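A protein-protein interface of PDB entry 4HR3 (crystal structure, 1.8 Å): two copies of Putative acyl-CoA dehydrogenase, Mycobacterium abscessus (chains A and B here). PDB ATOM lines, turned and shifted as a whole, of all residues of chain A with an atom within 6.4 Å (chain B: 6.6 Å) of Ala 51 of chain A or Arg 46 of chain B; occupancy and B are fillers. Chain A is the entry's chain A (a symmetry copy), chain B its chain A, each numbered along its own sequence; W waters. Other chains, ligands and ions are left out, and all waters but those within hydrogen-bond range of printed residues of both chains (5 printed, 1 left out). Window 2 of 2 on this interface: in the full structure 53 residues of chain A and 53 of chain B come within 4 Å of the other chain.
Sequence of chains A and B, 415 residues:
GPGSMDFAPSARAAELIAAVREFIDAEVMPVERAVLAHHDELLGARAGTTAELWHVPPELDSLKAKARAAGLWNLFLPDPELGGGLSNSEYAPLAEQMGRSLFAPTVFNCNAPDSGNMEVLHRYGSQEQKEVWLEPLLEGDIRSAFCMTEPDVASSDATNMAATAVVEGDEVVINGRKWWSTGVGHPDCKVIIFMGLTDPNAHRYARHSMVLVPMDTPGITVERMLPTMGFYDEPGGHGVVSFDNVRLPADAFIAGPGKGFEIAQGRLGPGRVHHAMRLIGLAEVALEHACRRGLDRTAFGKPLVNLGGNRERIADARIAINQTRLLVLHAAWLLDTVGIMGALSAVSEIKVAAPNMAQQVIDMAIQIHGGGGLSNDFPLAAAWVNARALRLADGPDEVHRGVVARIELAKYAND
The backbone carbonyl oxygen (O) of Leu 42 of chain B lies within hydrogen-bond range of the backbone NH (N) of Ala 47 of chain B, at 3.0 Å. OE1 of Glu 52 of chain A lies within hydrogen-bond range of N of Thr 49 of chain A (2.9 Å). The backbone NH (N) of Gly 185 of chain A lies within hydrogen-bond range of the backbone carbonyl oxygen (O) of Gly 236 of chain A (2.8 Å).
No position is printed for both chains. Of the 10 pairs that touch across the chains among the printed residues, none has its exchanged pair printed and touching as well.
Water W5 bridges the side-chain hydroxyl (OG1) of Thr 50 of chain A (2.5 Å) and the backbone carbonyl oxygen (O) of Ala 47 of chain B (2.6 Å). Water W4 lies within hydrogen-bond range of O of Gly 48 of chain B, N of Ala 51 of chain A, N of Thr 50 of chain A and O of Arg 46 of chain B. Water W1 bridges the backbone carbonyl oxygen (O) of Leu 43 of chain B and the indole nitrogen (NE1) of Trp 54 of chain A. Water W2 lies within hydrogen-bond range of NH2 of Arg 46 of chain B, O of Val 184 of chain A and O of Gly 185 of chain A. Water W3 bridges the backbone carbonyl oxygen of Gly 185 of chain A (3.3 Å) and the guanidinium group of Arg 46 of chain B (3.3 Å).
Arg 46 of chain B touches just these residues of chain A: Thr 50, Ala 51, Trp 54, Gly 185 and Met 225. Printed residues of chain A within 4 Å of Leu 43 of chain B: Thr 50 (3.6 Å). Printed residues of chain B within 4 Å of Thr 50 of chain A: Leu 43 (3.6 Å), Arg 46 (3.8 Å), Ala 47 (3.5 Å) and Gly 48 (3.0 Å). Of the printed residues of chain B, Gly 185 of chain A touches Arg 46. The nearest residue of chain B that does not touch Ala 51 of chain A is Gly 48 of chain B (4.5 Å). The nearest residue of chain A that does not touch Arg 46 of chain B is Pro 235 of chain A (4.6 Å). The nearest printed residue of chain B that does not touch Thr 50 of chain A is Leu 42 of chain B (4.8 Å).
Of the 15 printed residues of chain A, 6 touch a printed residue of chain B. Printed residues of chain A that touch a printed residue of chain B: Thr 49, Thr 50, Ala 51, Trp 54, Gly 185 and Met 225. Of the 8 printed residues of chain B, 5 touch a printed residue of chain A. Hydrophobic or aromatic side chains of chain B that line the printed part of chain A: Leu 43. Among the printed residues, 10 pairs touch across the chains. Among the printed residues, no Asp or Glu carboxylate lies within 4 Å of a Lys or Arg side-chain nitrogen of the other chain.
Among the printed residues, merely in contact across the chains: Thr 49 of chain A with Gly 48 of chain B (3.7 Å), Thr 50 of chain A with Leu 43 of chain B (3.6 Å), Thr 50 of chain A with Arg 46 of chain B (3.8 Å), Ala 51 of chain A with Arg 46 of chain B (3.6 Å), Trp 54 of chain A with Arg 46 of chain B (3.3 Å) and Met 225 of chain A with Arg 46 of chain B (3.6 Å).
The backbone carbonyl oxygen (O) of Gly 44 of chain B sits at hydrogen-bond distance from the backbone NH (N) of Met 225 of chain A. The backbone carbonyl oxygen (O) of Gly 185 of chain A sits at hydrogen-bond distance from the guanidinium group (NH1) of Arg 46 of chain B (2.8 Å). OG1 of Thr 50 of chain A sits close to O of Ala 47 of chain B (3.5 Å). O of Gly 48 of chain B lies within hydrogen-bond range of N of Thr 50 of chain A, at 3.0 Å.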
ATOM      1  N   THR A  49       9.257 -11.003 -23.880  1.00  0.00           N
ATOM      2  CA  THR A  49       8.321 -10.595 -22.851  1.00  0.00           C
ATOM      3  C   THR A  49       8.719  -9.228 -22.330  1.00  0.00           C
ATOM      4  O   THR A  49       9.870  -8.798 -22.453  1.00  0.00           O
ATOM      5  CB  THR A  49       8.305 -11.588 -21.662  1.00  0.00           C
ATOM      6  OG1 THR A  49       9.578 -11.569 -20.994  1.00  0.00           O
ATOM      7  CG2 THR A  49       7.996 -13.019 -22.134  1.00  0.00           C
ATOM      8  N   THR A  50       7.758  -8.544 -21.729  1.00  0.00           N
ATOM      9  CA  THR A  50       8.054  -7.313 -21.022  1.00  0.00           C
ATOM     10  C   THR A  50       8.903  -7.616 -19.793  1.00  0.00           C
ATOM     11  O   THR A  50       9.863  -6.903 -19.502  1.00  0.00           O
ATOM     12  CB  THR A  50       6.762  -6.574 -20.657  1.00  0.00           C
ATOM     13  OG1 THR A  50       6.167  -6.099 -21.865  1.00  0.00           O
ATOM     14  CG2 THR A  50       7.057  -5.379 -19.741  1.00  0.00           C
ATOM     15  N   ALA A  51       8.572  -8.693 -19.090  1.00  0.00           N
ATOM     16  CA  ALA A  51       9.279  -9.024 -17.853  1.00  0.00           C
ATOM     17  C   ALA A  51      10.782  -9.208 -18.064  1.00  0.00           C
ATOM     18  O   ALA A  51      11.563  -8.815 -17.212  1.00  0.00           O
ATOM     19  CB  ALA A  51       8.677 -10.262 -17.201  1.00  0.00           C
ATOM     20  N   GLU A  52      11.202  -9.782 -19.191  1.00  0.00           N
ATOM     21  CA  GLU A  52      12.639 -10.021 -19.388  1.00  0.00           C
ATOM     22  C   GLU A  52      13.471  -8.747 -19.539  1.00  0.00           C
ATOM     23  O   GLU A  52      14.670  -8.770 -19.302  1.00  0.00           O
ATOM     24  CB  GLU A  52      12.913 -10.972 -20.553  1.00  0.00           C
ATOM     25  CG  GLU A  52      12.750 -10.384 -21.944  1.00  0.00           C
ATOM     26  CD  GLU A  52      12.969 -11.433 -23.010  1.00  0.00           C
ATOM     27  OE1 GLU A  52      11.985 -11.840 -23.649  1.00  0.00           O
ATOM     28  OE2 GLU A  52      14.122 -11.890 -23.156  1.00  0.00           O
ATOM     29  N   LEU A  53      12.835  -7.638 -19.910  1.00  0.00           N
ATOM     30  CA  LEU A  53      13.525  -6.355 -20.020  1.00  0.00           C
ATOM     31  C   LEU A  53      13.981  -5.814 -18.661  1.00  0.00           C
ATOM     32  O   LEU A  53      14.834  -4.929 -18.595  1.00  0.00           O
ATOM     33  CB  LEU A  53      12.602  -5.327 -20.685  1.00  0.00           C
ATOM     34  CG  LEU A  53      12.046  -5.736 -22.055  1.00  0.00           C
ATOM     35  CD1 LEU A  53      10.948  -4.770 -22.496  1.00  0.00           C
ATOM     36  CD2 LEU A  53      13.154  -5.795 -23.089  1.00  0.00           C
ATOM     37  N   TRP A  54      13.404  -6.343 -17.588  1.00  0.00           N
ATOM     38  CA  TRP A  54      13.713  -5.919 -16.231  1.00  0.00           C
ATOM     39  C   TRP A  54      14.827  -6.732 -15.539  1.00  0.00           C
ATOM     40  O   TRP A  54      15.232  -6.402 -14.425  1.00  0.00           O
ATOM     41  CB  TRP A  54      12.428  -5.949 -15.401  1.00  0.00           C
ATOM     42  CG  TRP A  54      11.501  -4.860 -15.813  1.00  0.00           C
ATOM     43  CD1 TRP A  54      10.578  -4.896 -16.820  1.00  0.00           C
ATOM     44  CD2 TRP A  54      11.426  -3.553 -15.241  1.00  0.00           C
ATOM     45  NE1 TRP A  54       9.925  -3.690 -16.903  1.00  0.00           N
ATOM     46  CE2 TRP A  54      10.430  -2.846 -15.950  1.00  0.00           C
ATOM     47  CE3 TRP A  54      12.098  -2.914 -14.191  1.00  0.00           C
ATOM     48  CZ2 TRP A  54      10.078  -1.527 -15.632  1.00  0.00           C
ATOM     49  CZ3 TRP A  54      11.752  -1.601 -13.880  1.00  0.00           C
ATOM     50  CH2 TRP A  54      10.747  -0.925 -14.605  1.00  0.00           C
ATOM     51  N   HIS A  55      15.337  -7.771 -16.191  1.00  0.00           N
ATOM     52  CA  HIS A  55      16.408  -8.560 -15.585  1.00  0.00           C
ATOM     53  C   HIS A  55      17.617  -7.674 -15.296  1.00  0.00           C
ATOM     54  O   HIS A  55      17.982  -6.821 -16.092  1.00  0.00           O
ATOM     55  CB  HIS A  55      16.797  -9.757 -16.468  1.00  0.00           C
ATOM     56  CG  HIS A  55      15.731 -10.807 -16.570  1.00  0.00           C
ATOM     57  ND1 HIS A  55      15.703 -11.748 -17.580  1.00  0.00           N
ATOM     58  CD2 HIS A  55      14.647 -11.056 -15.797  1.00  0.00           C
ATOM     59  CE1 HIS A  55      14.659 -12.538 -17.417  1.00  0.00           C
ATOM     60  NE2 HIS A  55      13.998 -12.136 -16.345  1.00  0.00           N
ATOM     61  N   VAL A 184      12.722   1.185  -6.850  1.00  0.00           N
ATOM     62  CA  VAL A 184      11.897   0.180  -6.163  1.00  0.00           C
ATOM     63  C   VAL A 184      11.548  -1.029  -7.000  1.00  0.00           C
ATOM     64  O   VAL A 184      11.042  -2.012  -6.454  1.00  0.00           O
ATOM     65  CB  VAL A 184      10.557   0.721  -5.574  1.00  0.00           C
ATOM     66  CG1 VAL A 184      10.788   1.749  -4.495  1.00  0.00           C
ATOM     67  CG2 VAL A 184       9.626   1.270  -6.645  1.00  0.00           C
ATOM     68  N   GLY A 185      11.778  -0.973  -8.303  1.00  0.00           N
ATOM     69  CA  GLY A 185      11.560  -2.126  -9.168  1.00  0.00           C
ATOM     70  C   GLY A 185      12.656  -3.174  -9.103  1.00  0.00           C
ATOM     71  O   GLY A 185      12.485  -4.280  -9.610  1.00  0.00           O
ATOM     72  N   HIS A 186      13.795  -2.818  -8.508  1.00  0.00           N
ATOM     73  CA  HIS A 186      14.981  -3.681  -8.507  1.00  0.00           C
ATOM     74  C   HIS A 186      14.727  -4.843  -7.550  1.00  0.00           C
ATOM     75  O   HIS A 186      14.233  -4.602  -6.462  1.00  0.00           O
ATOM     76  CB  HIS A 186      16.183  -2.854  -8.028  1.00  0.00           C
ATOM     77  CG  HIS A 186      17.520  -3.440  -8.356  1.00  0.00           C
ATOM     78  ND1 HIS A 186      17.986  -4.604  -7.791  1.00  0.00           N
ATOM     79  CD2 HIS A 186      18.520  -2.983  -9.143  1.00  0.00           C
ATOM     80  CE1 HIS A 186      19.201  -4.855  -8.233  1.00  0.00           C
ATOM     81  NE2 HIS A 186      19.548  -3.888  -9.057  1.00  0.00           N
ATOM     82  N   PRO A 187      15.087  -6.084  -7.940  1.00  0.00           N
ATOM     83  CA  PRO A 187      14.901  -7.278  -7.086  1.00  0.00           C
ATOM     84  C   PRO A 187      15.619  -7.210  -5.744  1.00  0.00           C
ATOM     85  O   PRO A 187      15.224  -7.889  -4.788  1.00  0.00           O
ATOM     86  CB  PRO A 187      15.506  -8.424  -7.909  1.00  0.00           C
ATOM     87  CG  PRO A 187      15.686  -7.907  -9.271  1.00  0.00           C
ATOM     88  CD  PRO A 187      15.721  -6.422  -9.227  1.00  0.00           C
ATOM     89  N   VAL A 222       4.146  -2.574  -4.206  1.00  0.00           N
ATOM     90  CA  VAL A 222       4.634  -1.836  -5.356  1.00  0.00           C
ATOM     91  C   VAL A 222       3.546  -1.994  -6.425  1.00  0.00           C
ATOM     92  O   VAL A 222       3.371  -3.074  -6.990  1.00  0.00           O
ATOM     93  CB  VAL A 222       5.995  -2.358  -5.850  1.00  0.00           C
ATOM     94  CG1 VAL A 222       6.444  -1.580  -7.078  1.00  0.00           C
ATOM     95  CG2 VAL A 222       7.029  -2.269  -4.735  1.00  0.00           C
ATOM     96  N   MET A 225       5.066   0.379 -12.178  1.00  0.00           N
ATOM     97  CA  MET A 225       6.251   1.146 -12.572  1.00  0.00           C
ATOM     98  C   MET A 225       5.836   2.256 -13.539  1.00  0.00           C
ATOM     99  O   MET A 225       4.838   2.119 -14.241  1.00  0.00           O
ATOM    100  CB  MET A 225       7.282   0.228 -13.207  1.00  0.00           C
ATOM    101  CG  MET A 225       7.686  -0.965 -12.320  1.00  0.00           C
ATOM    102  SD  MET A 225       8.320  -0.499 -10.678  1.00  0.00           S
ATOM    103  CE  MET A 225       9.761   0.363 -11.184  1.00  0.00           C
ATOM    104  N   PRO A 235      16.905  -1.664 -14.545  1.00  0.00           N
ATOM    105  CA  PRO A 235      16.045  -2.552 -13.778  1.00  0.00           C
ATOM    106  C   PRO A 235      15.394  -1.954 -12.524  1.00  0.00           C
ATOM    107  O   PRO A 235      14.539  -2.597 -11.920  1.00  0.00           O
ATOM    108  CB  PRO A 235      17.006  -3.673 -13.389  1.00  0.00           C
ATOM    109  CG  PRO A 235      18.310  -2.955 -13.199  1.00  0.00           C
ATOM    110  CD  PRO A 235      18.338  -1.927 -14.276  1.00  0.00           C
ATOM    111  N   GLY A 236      15.811  -0.766 -12.118  1.00  0.00           N
ATOM    112  CA  GLY A 236      15.306  -0.146 -10.889  1.00  0.00           C
ATOM    113  C   GLY A 236      14.001   0.602 -11.076  1.00  0.00           C
ATOM    114  O   GLY A 236      13.148   0.633 -10.182  1.00  0.00           O
ATOM    115  N   GLU B  41      -1.045  -0.040 -18.460  1.00  0.00           N
ATOM    116  CA  GLU B  41      -1.267  -1.024 -17.410  1.00  0.00           C
ATOM    117  C   GLU B  41      -0.366  -2.244 -17.582  1.00  0.00           C
ATOM    118  O   GLU B  41       0.217  -2.725 -16.608  1.00  0.00           O
ATOM    119  CB  GLU B  41      -2.736  -1.484 -17.388  1.00  0.00           C
ATOM    120  N   LEU B  42      -0.262  -2.753 -18.808  1.00  0.00           N
ATOM    121  CA  LEU B  42       0.578  -3.924 -19.077  1.00  0.00           C
ATOM    122  C   LEU B  42       2.033  -3.614 -18.766  1.00  0.00           C
ATOM    123  O   LEU B  42       2.683  -4.351 -18.037  1.00  0.00           O
ATOM    124  CB  LEU B  42       0.459  -4.377 -20.527  1.00  0.00           C
ATOM    125  CG  LEU B  42      -0.787  -5.153 -20.923  1.00  0.00           C
ATOM    126  CD1 LEU B  42      -0.883  -5.275 -22.437  1.00  0.00           C
ATOM    127  CD2 LEU B  42      -0.772  -6.530 -20.281  1.00  0.00           C
ATOM    128  N   LEU B  43       2.539  -2.508 -19.301  1.00  0.00           N
ATOM    129  CA  LEU B  43       3.949  -2.167 -19.089  1.00  0.00           C
ATOM    130  C   LEU B  43       4.232  -1.826 -17.621  1.00  0.00           C
ATOM    131  O   LEU B  43       5.281  -2.189 -17.087  1.00  0.00           O
ATOM    132  CB  LEU B  43       4.395  -1.030 -20.007  1.00  0.00           C
ATOM    133  CG  LEU B  43       4.363  -1.374 -21.496  1.00  0.00           C
ATOM    134  CD1 LEU B  43       4.819  -0.194 -22.337  1.00  0.00           C
ATOM    135  CD2 LEU B  43       5.221  -2.597 -21.789  1.00  0.00           C
ATOM    136  N   GLY B  44       3.299  -1.130 -16.983  1.00  0.00           N
ATOM    137  CA  GLY B  44       3.416  -0.764 -15.578  1.00  0.00           C
ATOM    138  C   GLY B  44       3.460  -1.978 -14.663  1.00  0.00           C
ATOM    139  O   GLY B  44       4.080  -1.938 -13.603  1.00  0.00           O
ATOM    140  N   ALA B  45       2.811  -3.063 -15.086  1.00  0.00           N
ATOM    141  CA  ALA B  45       2.759  -4.298 -14.327  1.00  0.00           C
ATOM    142  C   ALA B  45       3.939  -5.214 -14.666  1.00  0.00           C
ATOM    143  O   ALA B  45       4.086  -6.295 -14.079  1.00  0.00           O
ATOM    144  CB  ALA B  45       1.443  -5.010 -14.613  1.00  0.00           C
ATOM    145  N   ARG B  46       4.785  -4.760 -15.589  1.00  0.00           N
ATOM    146  CA  ARG B  46       5.888  -5.547 -16.126  1.00  0.00           C
ATOM    147  C   ARG B  46       5.373  -6.895 -16.633  1.00  0.00           C
ATOM    148  O   ARG B  46       5.987  -7.937 -16.392  1.00  0.00           O
ATOM    149  CB  ARG B  46       6.998  -5.690 -15.073  1.00  0.00           C
ATOM    150  CG  ARG B  46       7.492  -4.329 -14.627  1.00  0.00           C
ATOM    151  CD  ARG B  46       8.670  -4.429 -13.669  1.00  0.00           C
ATOM    152  NE  ARG B  46       8.259  -4.517 -12.280  1.00  0.00           N
ATOM    153  CZ  ARG B  46       9.100  -4.607 -11.252  1.00  0.00           C
ATOM    154  NH1 ARG B  46      10.414  -4.677 -11.436  1.00  0.00           N
ATOM    155  NH2 ARG B  46       8.612  -4.639 -10.023  1.00  0.00           N
ATOM    156  N   ALA B  47       4.234  -6.854 -17.327  1.00  0.00           N
ATOM    157  CA  ALA B  47       3.506  -8.051 -17.717  1.00  0.00           C
ATOM    158  C   ALA B  47       3.298  -8.145 -19.223  1.00  0.00           C
ATOM    159  O   ALA B  47       3.432  -7.155 -19.955  1.00  0.00           O
ATOM    160  CB  ALA B  47       2.152  -8.091 -17.021  1.00  0.00           C
ATOM    161  N   GLY B  48       2.951  -9.350 -19.666  1.00  0.00           N
ATOM    162  CA  GLY B  48       2.588  -9.600 -21.051  1.00  0.00           C
ATOM    163  C   GLY B  48       3.767  -9.660 -21.997  1.00  0.00           C
ATOM    164  O   GLY B  48       4.930  -9.634 -21.578  1.00  0.00           O
HETATM  165  O   HOH W   1       7.736  -2.524 -18.343  1.00  0.00           O
HETATM  166  O   HOH W   2       9.922  -5.009  -7.522  1.00  0.00           O
HETATM  167  O   HOH W   3      12.562  -7.221 -11.133  1.00  0.00           O
HETATM  168  O   HOH W   4       6.123 -10.056 -19.135  1.00  0.00           O
HETATM  169  O   HOH W   5       3.683  -6.231 -22.379  1.00  0.00           O
